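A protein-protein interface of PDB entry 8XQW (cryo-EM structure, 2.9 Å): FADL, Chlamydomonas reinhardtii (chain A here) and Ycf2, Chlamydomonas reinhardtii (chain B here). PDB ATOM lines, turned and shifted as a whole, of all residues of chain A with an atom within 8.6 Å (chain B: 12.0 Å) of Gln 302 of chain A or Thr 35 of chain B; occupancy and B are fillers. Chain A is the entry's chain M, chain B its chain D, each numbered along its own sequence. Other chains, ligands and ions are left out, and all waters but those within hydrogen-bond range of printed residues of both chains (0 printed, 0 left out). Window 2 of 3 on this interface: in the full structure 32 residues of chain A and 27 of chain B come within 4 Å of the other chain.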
ATOM      1  N   SER A 297      -7.342 -17.553  -4.940  1.00  0.00           N
ATOM      2  CA  SER A 297      -6.789 -16.591  -4.001  1.00  0.00           C
ATOM      3  C   SER A 297      -5.275 -16.684  -3.913  1.00  0.00           C
ATOM      4  O   SER A 297      -4.645 -15.796  -3.333  1.00  0.00           O
ATOM      5  CB  SER A 297      -7.394 -16.798  -2.618  1.00  0.00           C
ATOM      6  OG  SER A 297      -6.466 -16.435  -1.615  1.00  0.00           O
ATOM      7  N   GLN A 298      -4.682 -17.746  -4.458  1.00  0.00           N
ATOM      8  CA  GLN A 298      -3.235 -17.871  -4.503  1.00  0.00           C
ATOM      9  C   GLN A 298      -2.626 -17.131  -5.683  1.00  0.00           C
ATOM     10  O   GLN A 298      -1.407 -16.941  -5.714  1.00  0.00           O
ATOM     11  CB  GLN A 298      -2.840 -19.339  -4.583  1.00  0.00           C
ATOM     12  CG  GLN A 298      -3.084 -19.932  -5.947  1.00  0.00           C
ATOM     13  CD  GLN A 298      -3.175 -21.435  -5.922  1.00  0.00           C
ATOM     14  OE1 GLN A 298      -3.107 -22.057  -4.863  1.00  0.00           O
ATOM     15  NE2 GLN A 298      -3.333 -22.033  -7.092  1.00  0.00           N
ATOM     16  N   LEU A 299      -3.441 -16.727  -6.659  1.00  0.00           N
ATOM     17  CA  LEU A 299      -2.934 -15.972  -7.794  1.00  0.00           C
ATOM     18  C   LEU A 299      -2.768 -14.496  -7.476  1.00  0.00           C
ATOM     19  O   LEU A 299      -2.357 -13.729  -8.349  1.00  0.00           O
ATOM     20  CB  LEU A 299      -3.869 -16.131  -8.989  1.00  0.00           C
ATOM     21  CG  LEU A 299      -4.343 -17.546  -9.304  1.00  0.00           C
ATOM     22  CD1 LEU A 299      -5.186 -17.544 -10.555  1.00  0.00           C
ATOM     23  CD2 LEU A 299      -3.161 -18.468  -9.472  1.00  0.00           C
ATOM     24  N   LEU A 300      -3.086 -14.083  -6.266  1.00  0.00           N
ATOM     25  CA  LEU A 300      -3.078 -12.667  -5.933  1.00  0.00           C
ATOM     26  C   LEU A 300      -1.794 -12.301  -5.199  1.00  0.00           C
ATOM     27  O   LEU A 300      -1.370 -13.034  -4.305  1.00  0.00           O
ATOM     28  CB  LEU A 300      -4.282 -12.320  -5.071  1.00  0.00           C
ATOM     29  CG  LEU A 300      -5.419 -11.554  -5.740  1.00  0.00           C
ATOM     30  CD1 LEU A 300      -5.759 -12.151  -7.086  1.00  0.00           C
ATOM     31  CD2 LEU A 300      -6.628 -11.570  -4.841  1.00  0.00           C
ATOM     32  N   PRO A 301      -1.156 -11.189  -5.549  1.00  0.00           N
ATOM     33  CA  PRO A 301      -0.019 -10.711  -4.762  1.00  0.00           C
ATOM     34  C   PRO A 301      -0.437 -10.367  -3.343  1.00  0.00           C
ATOM     35  O   PRO A 301      -1.548  -9.909  -3.086  1.00  0.00           O
ATOM     36  CB  PRO A 301       0.438  -9.464  -5.522  1.00  0.00           C
ATOM     37  CG  PRO A 301      -0.055  -9.669  -6.906  1.00  0.00           C
ATOM     38  CD  PRO A 301      -1.343 -10.409  -6.781  1.00  0.00           C
ATOM     39  N   GLN A 302       0.487 -10.587  -2.413  1.00  0.00           N
ATOM     40  CA  GLN A 302       0.195 -10.381  -1.003  1.00  0.00           C
ATOM     41  C   GLN A 302       0.085  -8.911  -0.633  1.00  0.00           C
ATOM     42  O   GLN A 302      -0.448  -8.593   0.433  1.00  0.00           O
ATOM     43  CB  GLN A 302       1.274 -11.044  -0.150  1.00  0.00           C
ATOM     44  CG  GLN A 302       0.888 -11.245   1.297  1.00  0.00           C
ATOM     45  CD  GLN A 302       1.435 -10.167   2.202  1.00  0.00           C
ATOM     46  OE1 GLN A 302       2.012  -9.184   1.737  1.00  0.00           O
ATOM     47  NE2 GLN A 302       1.259 -10.342   3.505  1.00  0.00           N
ATOM     48  N   ALA A 303       0.572  -8.010  -1.484  1.00  0.00           N
ATOM     49  CA  ALA A 303       0.489  -6.588  -1.173  1.00  0.00           C
ATOM     50  C   ALA A 303      -0.928  -6.058  -1.331  1.00  0.00           C
ATOM     51  O   ALA A 303      -1.232  -4.958  -0.861  1.00  0.00           O
ATOM     52  CB  ALA A 303       1.445  -5.800  -2.064  1.00  0.00           C
ATOM     53  N   LEU A 304      -1.802  -6.818  -1.993  1.00  0.00           N
ATOM     54  CA  LEU A 304      -3.159  -6.346  -2.231  1.00  0.00           C
ATOM     55  C   LEU A 304      -3.968  -6.309  -0.943  1.00  0.00           C
ATOM     56  O   LEU A 304      -4.965  -5.586  -0.848  1.00  0.00           O
ATOM     57  CB  LEU A 304      -3.838  -7.234  -3.268  1.00  0.00           C
ATOM     58  CG  LEU A 304      -3.340  -7.040  -4.693  1.00  0.00           C
ATOM     59  CD1 LEU A 304      -4.076  -7.949  -5.632  1.00  0.00           C
ATOM     60  CD2 LEU A 304      -3.531  -5.604  -5.105  1.00  0.00           C
ATOM     61  N   PHE A 305      -3.558  -7.070   0.053  1.00  0.00           N
ATOM     62  CA  PHE A 305      -4.302  -7.161   1.302  1.00  0.00           C
ATOM     63  C   PHE A 305      -3.890  -6.138   2.319  1.00  0.00           C
ATOM     64  O   PHE A 305      -4.341  -6.248   3.457  1.00  0.00           O
ATOM     65  CB  PHE A 305      -4.143  -8.559   1.899  1.00  0.00           C
ATOM     66  CG  PHE A 305      -4.780  -9.642   1.086  1.00  0.00           C
ATOM     67  CD1 PHE A 305      -4.142 -10.160  -0.018  1.00  0.00           C
ATOM     68  CD2 PHE A 305      -6.010 -10.149   1.433  1.00  0.00           C
ATOM     69  CE1 PHE A 305      -4.721 -11.154  -0.760  1.00  0.00           C
ATOM     70  CE2 PHE A 305      -6.589 -11.146   0.691  1.00  0.00           C
ATOM     71  CZ  PHE A 305      -5.943 -11.647  -0.406  1.00  0.00           C
ATOM     72  N   ALA A 306      -3.080  -5.138   2.005  1.00  0.00           N
ATOM     73  CA  ALA A 306      -2.533  -4.243   3.013  1.00  0.00           C
ATOM     74  C   ALA A 306      -3.528  -3.147   3.360  1.00  0.00           C
ATOM     75  O   ALA A 306      -4.290  -2.689   2.506  1.00  0.00           O
ATOM     76  CB  ALA A 306      -1.226  -3.619   2.530  1.00  0.00           C
ATOM     77  N   PHE A 307      -3.510  -2.723   4.618  1.00  0.00           N
ATOM     78  CA  PHE A 307      -4.388  -1.649   5.049  1.00  0.00           C
ATOM     79  C   PHE A 307      -3.682  -0.303   4.982  1.00  0.00           C
ATOM     80  O   PHE A 307      -2.517  -0.164   5.361  1.00  0.00           O
ATOM     81  CB  PHE A 307      -4.877  -1.897   6.469  1.00  0.00           C
ATOM     82  CG  PHE A 307      -5.739  -0.801   7.003  1.00  0.00           C
ATOM     83  CD1 PHE A 307      -7.031  -0.648   6.557  1.00  0.00           C
ATOM     84  CD2 PHE A 307      -5.262   0.070   7.955  1.00  0.00           C
ATOM     85  CE1 PHE A 307      -7.828   0.355   7.042  1.00  0.00           C
ATOM     86  CE2 PHE A 307      -6.061   1.073   8.448  1.00  0.00           C
ATOM     87  CZ  PHE A 307      -7.343   1.215   7.989  1.00  0.00           C
ATOM     88  N   ASP A 308      -4.412   0.703   4.503  1.00  0.00           N
ATOM     89  CA  ASP A 308      -3.907   2.063   4.432  1.00  0.00           C
ATOM     90  C   ASP A 308      -5.049   3.015   4.738  1.00  0.00           C
ATOM     91  O   ASP A 308      -6.182   2.785   4.315  1.00  0.00           O
ATOM     92  CB  ASP A 308      -3.313   2.373   3.058  1.00  0.00           C
ATOM     93  CG  ASP A 308      -4.341   2.321   1.964  1.00  0.00           C
ATOM     94  OD1 ASP A 308      -5.212   1.435   2.029  1.00  0.00           O
ATOM     95  OD2 ASP A 308      -4.285   3.160   1.043  1.00  0.00           O
ATOM     96  N   GLN A 371      -8.878  -3.807  12.580  1.00  0.00           N
ATOM     97  CA  GLN A 371      -8.188  -3.536  13.837  1.00  0.00           C
ATOM     98  C   GLN A 371      -9.157  -3.041  14.898  1.00  0.00           C
ATOM     99  O   GLN A 371      -9.050  -3.401  16.073  1.00  0.00           O
ATOM    100  CB  GLN A 371      -7.076  -2.517  13.616  1.00  0.00           C
ATOM    101  CG  GLN A 371      -6.079  -2.928  12.579  1.00  0.00           C
ATOM    102  CD  GLN A 371      -6.488  -2.481  11.211  1.00  0.00           C
ATOM    103  OE1 GLN A 371      -7.103  -1.429  11.053  1.00  0.00           O
ATOM    104  NE2 GLN A 371      -6.157  -3.278  10.205  1.00  0.00           N
ATOM    105  N   GLY A 579     -11.486 -11.787   1.863  1.00  0.00           N
ATOM    106  CA  GLY A 579     -10.882 -10.778   2.704  1.00  0.00           C
ATOM    107  C   GLY A 579     -10.246  -9.637   1.949  1.00  0.00           C
ATOM    108  O   GLY A 579      -9.636  -8.764   2.579  1.00  0.00           O
ATOM    109  N   LEU A 580     -10.363  -9.600   0.645  1.00  0.00           N
ATOM    110  CA  LEU A 580      -9.707  -8.581  -0.154  1.00  0.00           C
ATOM    111  C   LEU A 580     -10.393  -7.239   0.053  1.00  0.00           C
ATOM    112  O   LEU A 580     -11.576  -7.107  -0.261  1.00  0.00           O
ATOM    113  CB  LEU A 580      -9.752  -8.970  -1.619  1.00  0.00           C
ATOM    114  CG  LEU A 580      -9.115  -8.015  -2.608  1.00  0.00           C
ATOM    115  CD1 LEU A 580      -7.640  -7.948  -2.354  1.00  0.00           C
ATOM    116  CD2 LEU A 580      -9.397  -8.483  -4.010  1.00  0.00           C
ATOM    117  N   PRO A 581      -9.689  -6.226   0.550  1.00  0.00           N
ATOM    118  CA  PRO A 581     -10.337  -4.941   0.835  1.00  0.00           C
ATOM    119  C   PRO A 581     -10.907  -4.269  -0.398  1.00  0.00           C
ATOM    120  O   PRO A 581     -10.685  -4.711  -1.525  1.00  0.00           O
ATOM    121  CB  PRO A 581      -9.208  -4.110   1.449  1.00  0.00           C
ATOM    122  CG  PRO A 581      -7.982  -4.738   0.964  1.00  0.00           C
ATOM    123  CD  PRO A 581      -8.264  -6.196   0.897  1.00  0.00           C
ATOM    124  N   SER A 584      -8.611  -2.353  -3.262  1.00  0.00           N
ATOM    125  CA  SER A 584      -7.755  -3.207  -4.063  1.00  0.00           C
ATOM    126  C   SER A 584      -8.532  -4.039  -5.066  1.00  0.00           C
ATOM    127  O   SER A 584      -7.957  -4.937  -5.681  1.00  0.00           O
ATOM    128  CB  SER A 584      -6.939  -4.129  -3.160  1.00  0.00           C
ATOM    129  OG  SER A 584      -6.595  -3.475  -1.954  1.00  0.00           O
ATOM    130  N   THR B  35      -1.325  -5.919   6.711  1.00  0.00           N
ATOM    131  CA  THR B  35      -1.461  -6.938   5.680  1.00  0.00           C
ATOM    132  C   THR B  35      -1.775  -8.298   6.273  1.00  0.00           C
ATOM    133  O   THR B  35      -1.954  -9.274   5.550  1.00  0.00           O
ATOM    134  CB  THR B  35      -0.191  -7.057   4.837  1.00  0.00           C
ATOM    135  OG1 THR B  35      -0.208  -8.300   4.129  1.00  0.00           O
ATOM    136  CG2 THR B  35       1.032  -7.007   5.727  1.00  0.00           C
ATOM    137  N   LEU B  36      -1.830  -8.363   7.599  1.00  0.00           N
ATOM    138  CA  LEU B  36      -2.139  -9.615   8.273  1.00  0.00           C
ATOM    139  C   LEU B  36      -3.566  -9.660   8.792  1.00  0.00           C
ATOM    140  O   LEU B  36      -4.183 -10.735   8.797  1.00  0.00           O
ATOM    141  CB  LEU B  36      -1.165  -9.849   9.429  1.00  0.00           C
ATOM    142  CG  LEU B  36       0.137 -10.570   9.075  1.00  0.00           C
ATOM    143  CD1 LEU B  36      -0.153 -11.848   8.303  1.00  0.00           C
ATOM    144  CD2 LEU B  36       1.075  -9.668   8.294  1.00  0.00           C
ATOM    145  N   GLN B  37      -4.106  -8.517   9.218  1.00  0.00           N
ATOM    146  CA  GLN B  37      -5.471  -8.495   9.726  1.00  0.00           C
ATOM    147  C   GLN B  37      -6.472  -8.842   8.635  1.00  0.00           C
ATOM    148  O   GLN B  37      -7.549  -9.370   8.925  1.00  0.00           O
ATOM    149  CB  GLN B  37      -5.786  -7.132  10.331  1.00  0.00           C
ATOM    150  CG  GLN B  37      -5.296  -6.974  11.752  1.00  0.00           C
ATOM    151  CD  GLN B  37      -6.281  -7.504  12.772  1.00  0.00           C
ATOM    152  OE1 GLN B  37      -6.857  -6.740  13.546  1.00  0.00           O
ATOM    153  NE2 GLN B  37      -6.478  -8.818  12.784  1.00  0.00           N
ATOM    154  N   ASN B  38      -6.139  -8.562   7.378  1.00  0.00           N
ATOM    155  CA  ASN B  38      -7.034  -8.955   6.301  1.00  0.00           C
ATOM    156  C   ASN B  38      -6.772 -10.380   5.834  1.00  0.00           C
ATOM    157  O   ASN B  38      -7.711 -11.076   5.445  1.00  0.00           O
ATOM    158  CB  ASN B  38      -6.918  -7.975   5.137  1.00  0.00           C
ATOM    159  CG  ASN B  38      -7.982  -6.893   5.180  1.00  0.00           C
ATOM    160  OD1 ASN B  38      -8.850  -6.824   4.316  1.00  0.00           O
ATOM    161  ND2 ASN B  38      -7.922  -6.049   6.198  1.00  0.00           N
ATOM    162  N   GLU B  39      -5.525 -10.842   5.880  1.00  0.00           N
ATOM    163  CA  GLU B  39      -5.242 -12.211   5.460  1.00  0.00           C
ATOM    164  C   GLU B  39      -5.837 -13.225   6.427  1.00  0.00           C
ATOM    165  O   GLU B  39      -6.290 -14.299   6.010  1.00  0.00           O
ATOM    166  CB  GLU B  39      -3.739 -12.417   5.330  1.00  0.00           C
ATOM    167  CG  GLU B  39      -3.155 -11.852   4.062  1.00  0.00           C
ATOM    168  CD  GLU B  39      -2.077 -12.736   3.481  1.00  0.00           C
ATOM    169  OE1 GLU B  39      -2.419 -13.782   2.896  1.00  0.00           O
ATOM    170  OE2 GLU B  39      -0.887 -12.390   3.619  1.00  0.00           O
ATOM    171  N   ARG B  40      -5.841 -12.904   7.723  1.00  0.00           N
ATOM    172  CA  ARG B  40      -6.497 -13.764   8.702  1.00  0.00           C
ATOM    173  C   ARG B  40      -7.977 -13.932   8.384  1.00  0.00           C
ATOM    174  O   ARG B  40      -8.494 -15.058   8.326  1.00  0.00           O
ATOM    175  CB  ARG B  40      -6.309 -13.181  10.099  1.00  0.00           C
ATOM    176  CG  ARG B  40      -7.200 -13.794  11.148  1.00  0.00           C
ATOM    177  CD  ARG B  40      -6.730 -13.435  12.549  1.00  0.00           C
ATOM    178  NE  ARG B  40      -7.790 -13.619  13.537  1.00  0.00           N
ATOM    179  CZ  ARG B  40      -8.605 -12.654  13.947  1.00  0.00           C
ATOM    180  NH1 ARG B  40      -9.543 -12.913  14.847  1.00  0.00           N
ATOM    181  NH2 ARG B  40      -8.484 -11.426  13.460  1.00  0.00           N
ATOM    182  N   ILE B  41      -8.678 -12.812   8.180  1.00  0.00           N
ATOM    183  CA  ILE B  41     -10.086 -12.856   7.814  1.00  0.00           C
ATOM    184  C   ILE B  41     -10.278 -13.626   6.521  1.00  0.00           C
ATOM    185  O   ILE B  41     -11.222 -14.415   6.391  1.00  0.00           O
ATOM    186  CB  ILE B  41     -10.647 -11.427   7.702  1.00  0.00           C
ATOM    187  CG1 ILE B  41     -10.568 -10.715   9.051  1.00  0.00           C
ATOM    188  CG2 ILE B  41     -12.080 -11.452   7.219  1.00  0.00           C
ATOM    189  CD1 ILE B  41     -11.373 -11.382  10.133  1.00  0.00           C
ATOM    190  N   ASN B  42      -9.388 -13.425   5.554  1.00  0.00           N
ATOM    191  CA  ASN B  42      -9.516 -14.105   4.273  1.00  0.00           C
ATOM    192  C   ASN B  42      -9.466 -15.615   4.450  1.00  0.00           C
ATOM    193  O   ASN B  42     -10.336 -16.338   3.951  1.00  0.00           O
ATOM    194  CB  ASN B  42      -8.416 -13.629   3.329  1.00  0.00           C
ATOM    195  CG  ASN B  42      -8.341 -14.444   2.066  1.00  0.00           C
ATOM    196  OD1 ASN B  42      -7.755 -15.521   2.041  1.00  0.00           O
ATOM    197  ND2 ASN B  42      -8.926 -13.929   1.002  1.00  0.00           N
ATOM    198  N   LYS B  43      -8.461 -16.110   5.169  1.00  0.00           N
ATOM    199  CA  LYS B  43      -8.338 -17.556   5.311  1.00  0.00           C
ATOM    200  C   LYS B  43      -9.467 -18.139   6.151  1.00  0.00           C
ATOM    201  O   LYS B  43      -9.942 -19.245   5.859  1.00  0.00           O
ATOM    202  CB  LYS B  43      -6.969 -17.917   5.887  1.00  0.00           C
ATOM    203  CG  LYS B  43      -6.875 -17.903   7.393  1.00  0.00           C
ATOM    204  CD  LYS B  43      -5.432 -18.012   7.851  1.00  0.00           C
ATOM    205  CE  LYS B  43      -4.632 -16.781   7.452  1.00  0.00           C
ATOM    206  NZ  LYS B  43      -3.556 -16.469   8.435  1.00  0.00           N
ATOM    207  N   GLN B  44      -9.943 -17.411   7.164  1.00  0.00           N
ATOM    208  CA  GLN B  44     -11.066 -17.911   7.953  1.00  0.00           C
ATOM    209  C   GLN B  44     -12.321 -18.042   7.100  1.00  0.00           C
ATOM    210  O   GLN B  44     -12.995 -19.083   7.112  1.00  0.00           O
ATOM    211  CB  GLN B  44     -11.326 -16.994   9.143  1.00  0.00           C
ATOM    212  CG  GLN B  44     -10.314 -17.126  10.253  1.00  0.00           C
ATOM    213  CD  GLN B  44     -10.589 -16.172  11.391  1.00  0.00           C
ATOM    214  OE1 GLN B  44     -10.226 -16.431  12.536  1.00  0.00           O
ATOM    215  NE2 GLN B  44     -11.239 -15.062  11.083  1.00  0.00           N
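Among the printed residues, pairs that only touch across the chains: Ser 297 of chain A with Asn 42 of chain B, Phe 305 of chain A with Thr 35 of chain B, Phe 305 of chain A with Asn 38 of chain B, Phe 305 of chain A with Asn 42 of chain B, Ala 306 of chain A with Thr 35 of chain B, Gln 371 of chain A with Gln 37 of chain B and Pro 581 of chain A with Asn 38 of chain B.
Gln 302 of chain A touches just these residues of chain B: Thr 35 (2.6 Å) and Glu 39 (3.0 Å). Thr 35 of chain B touches just these residues of chain A: Gln 302, Phe 305 and Ala 306. No residue of chain B comes within 4 Å of Pro 301 of chain A. No residue of chain B comes within 4 Å of Ala 303 of chain A. No residue of chain B comes within 4 Å of Leu 304 of chain A. Of chain B, only Thr 35 (3.7 Å), Asn 38 (3.5 Å) and Asn 42 (3.6 Å) come within 4 Å of Phe 305 of chain A. No residue of chain A comes within 4 Å of Leu 36 of chain B. Of the printed residues of chain A, Asn 38 of chain B touches Phe 305, Gly 579 and Pro 581. Of the printed residues of chain B, Gly 579 of chain A touches Asn 38 and Asn 42. Printed residues of chain A within 4 Å of Asn 42 of chain B: Ser 297, Phe 305 and Gly 579. Printed residues of chain A within 4 Å of Gln 37 of chain B: Gln 371. Of the printed residues of chain B, Ser 297 of chain A touches Asn 42. Ser 584 of chain A touches none of the printed residues of chain B. Asp 308 of chain A touches none of the printed residues of chain B. The nearest residue of chain B that does not touch Gln 302 of chain A is Leu 36 of chain B (4.8 Å). The nearest printed residue of chain B that does not touch Gln 371 of chain A is Asn 38 of chain B (5.2 Å).
Printed residues of chain B that touch a printed residue of chain A: Thr 35, Gln 37, Asn 38, Glu 39 and Asn 42. Printed residues of chain A that touch a printed residue of chain B: Ser 297, Gln 302, Phe 305, Ala 306, Gln 371, Gly 579 and Pro 581. Hydrophobic or aromatic side chains of chain A that line the printed part of chain B: Phe 305 and Pro 581. Among the printed residues, no Asp or Glu carboxylate lies within 4 Å of a Lys or Arg side-chain nitrogen of the other chain.
The side-chain hydroxyl of Thr 35 of chain B is in hydrogen-bond range of the side-chain amide nitrogen of Gln 302 of chain A (2.6 Å). The side-chain amide nitrogen (NE2) of Gln 302 of chain A lies within hydrogen-bond range of the side-chain carboxylate (OE2) of Glu 39 of chain B (3.0 Å). The backbone NH (N) of Gly 579 of chain A lies close to the side-chain amide nitrogen (ND2) of Asn 42 of chain B (3.4 Å). O of Gly 579 of chain A sits close to OD1 of Asn 38 of chain B, 2.7 Å away.
NH2 of Arg 40 of chain B lies close to NE2 of Gln 37 of chain B.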
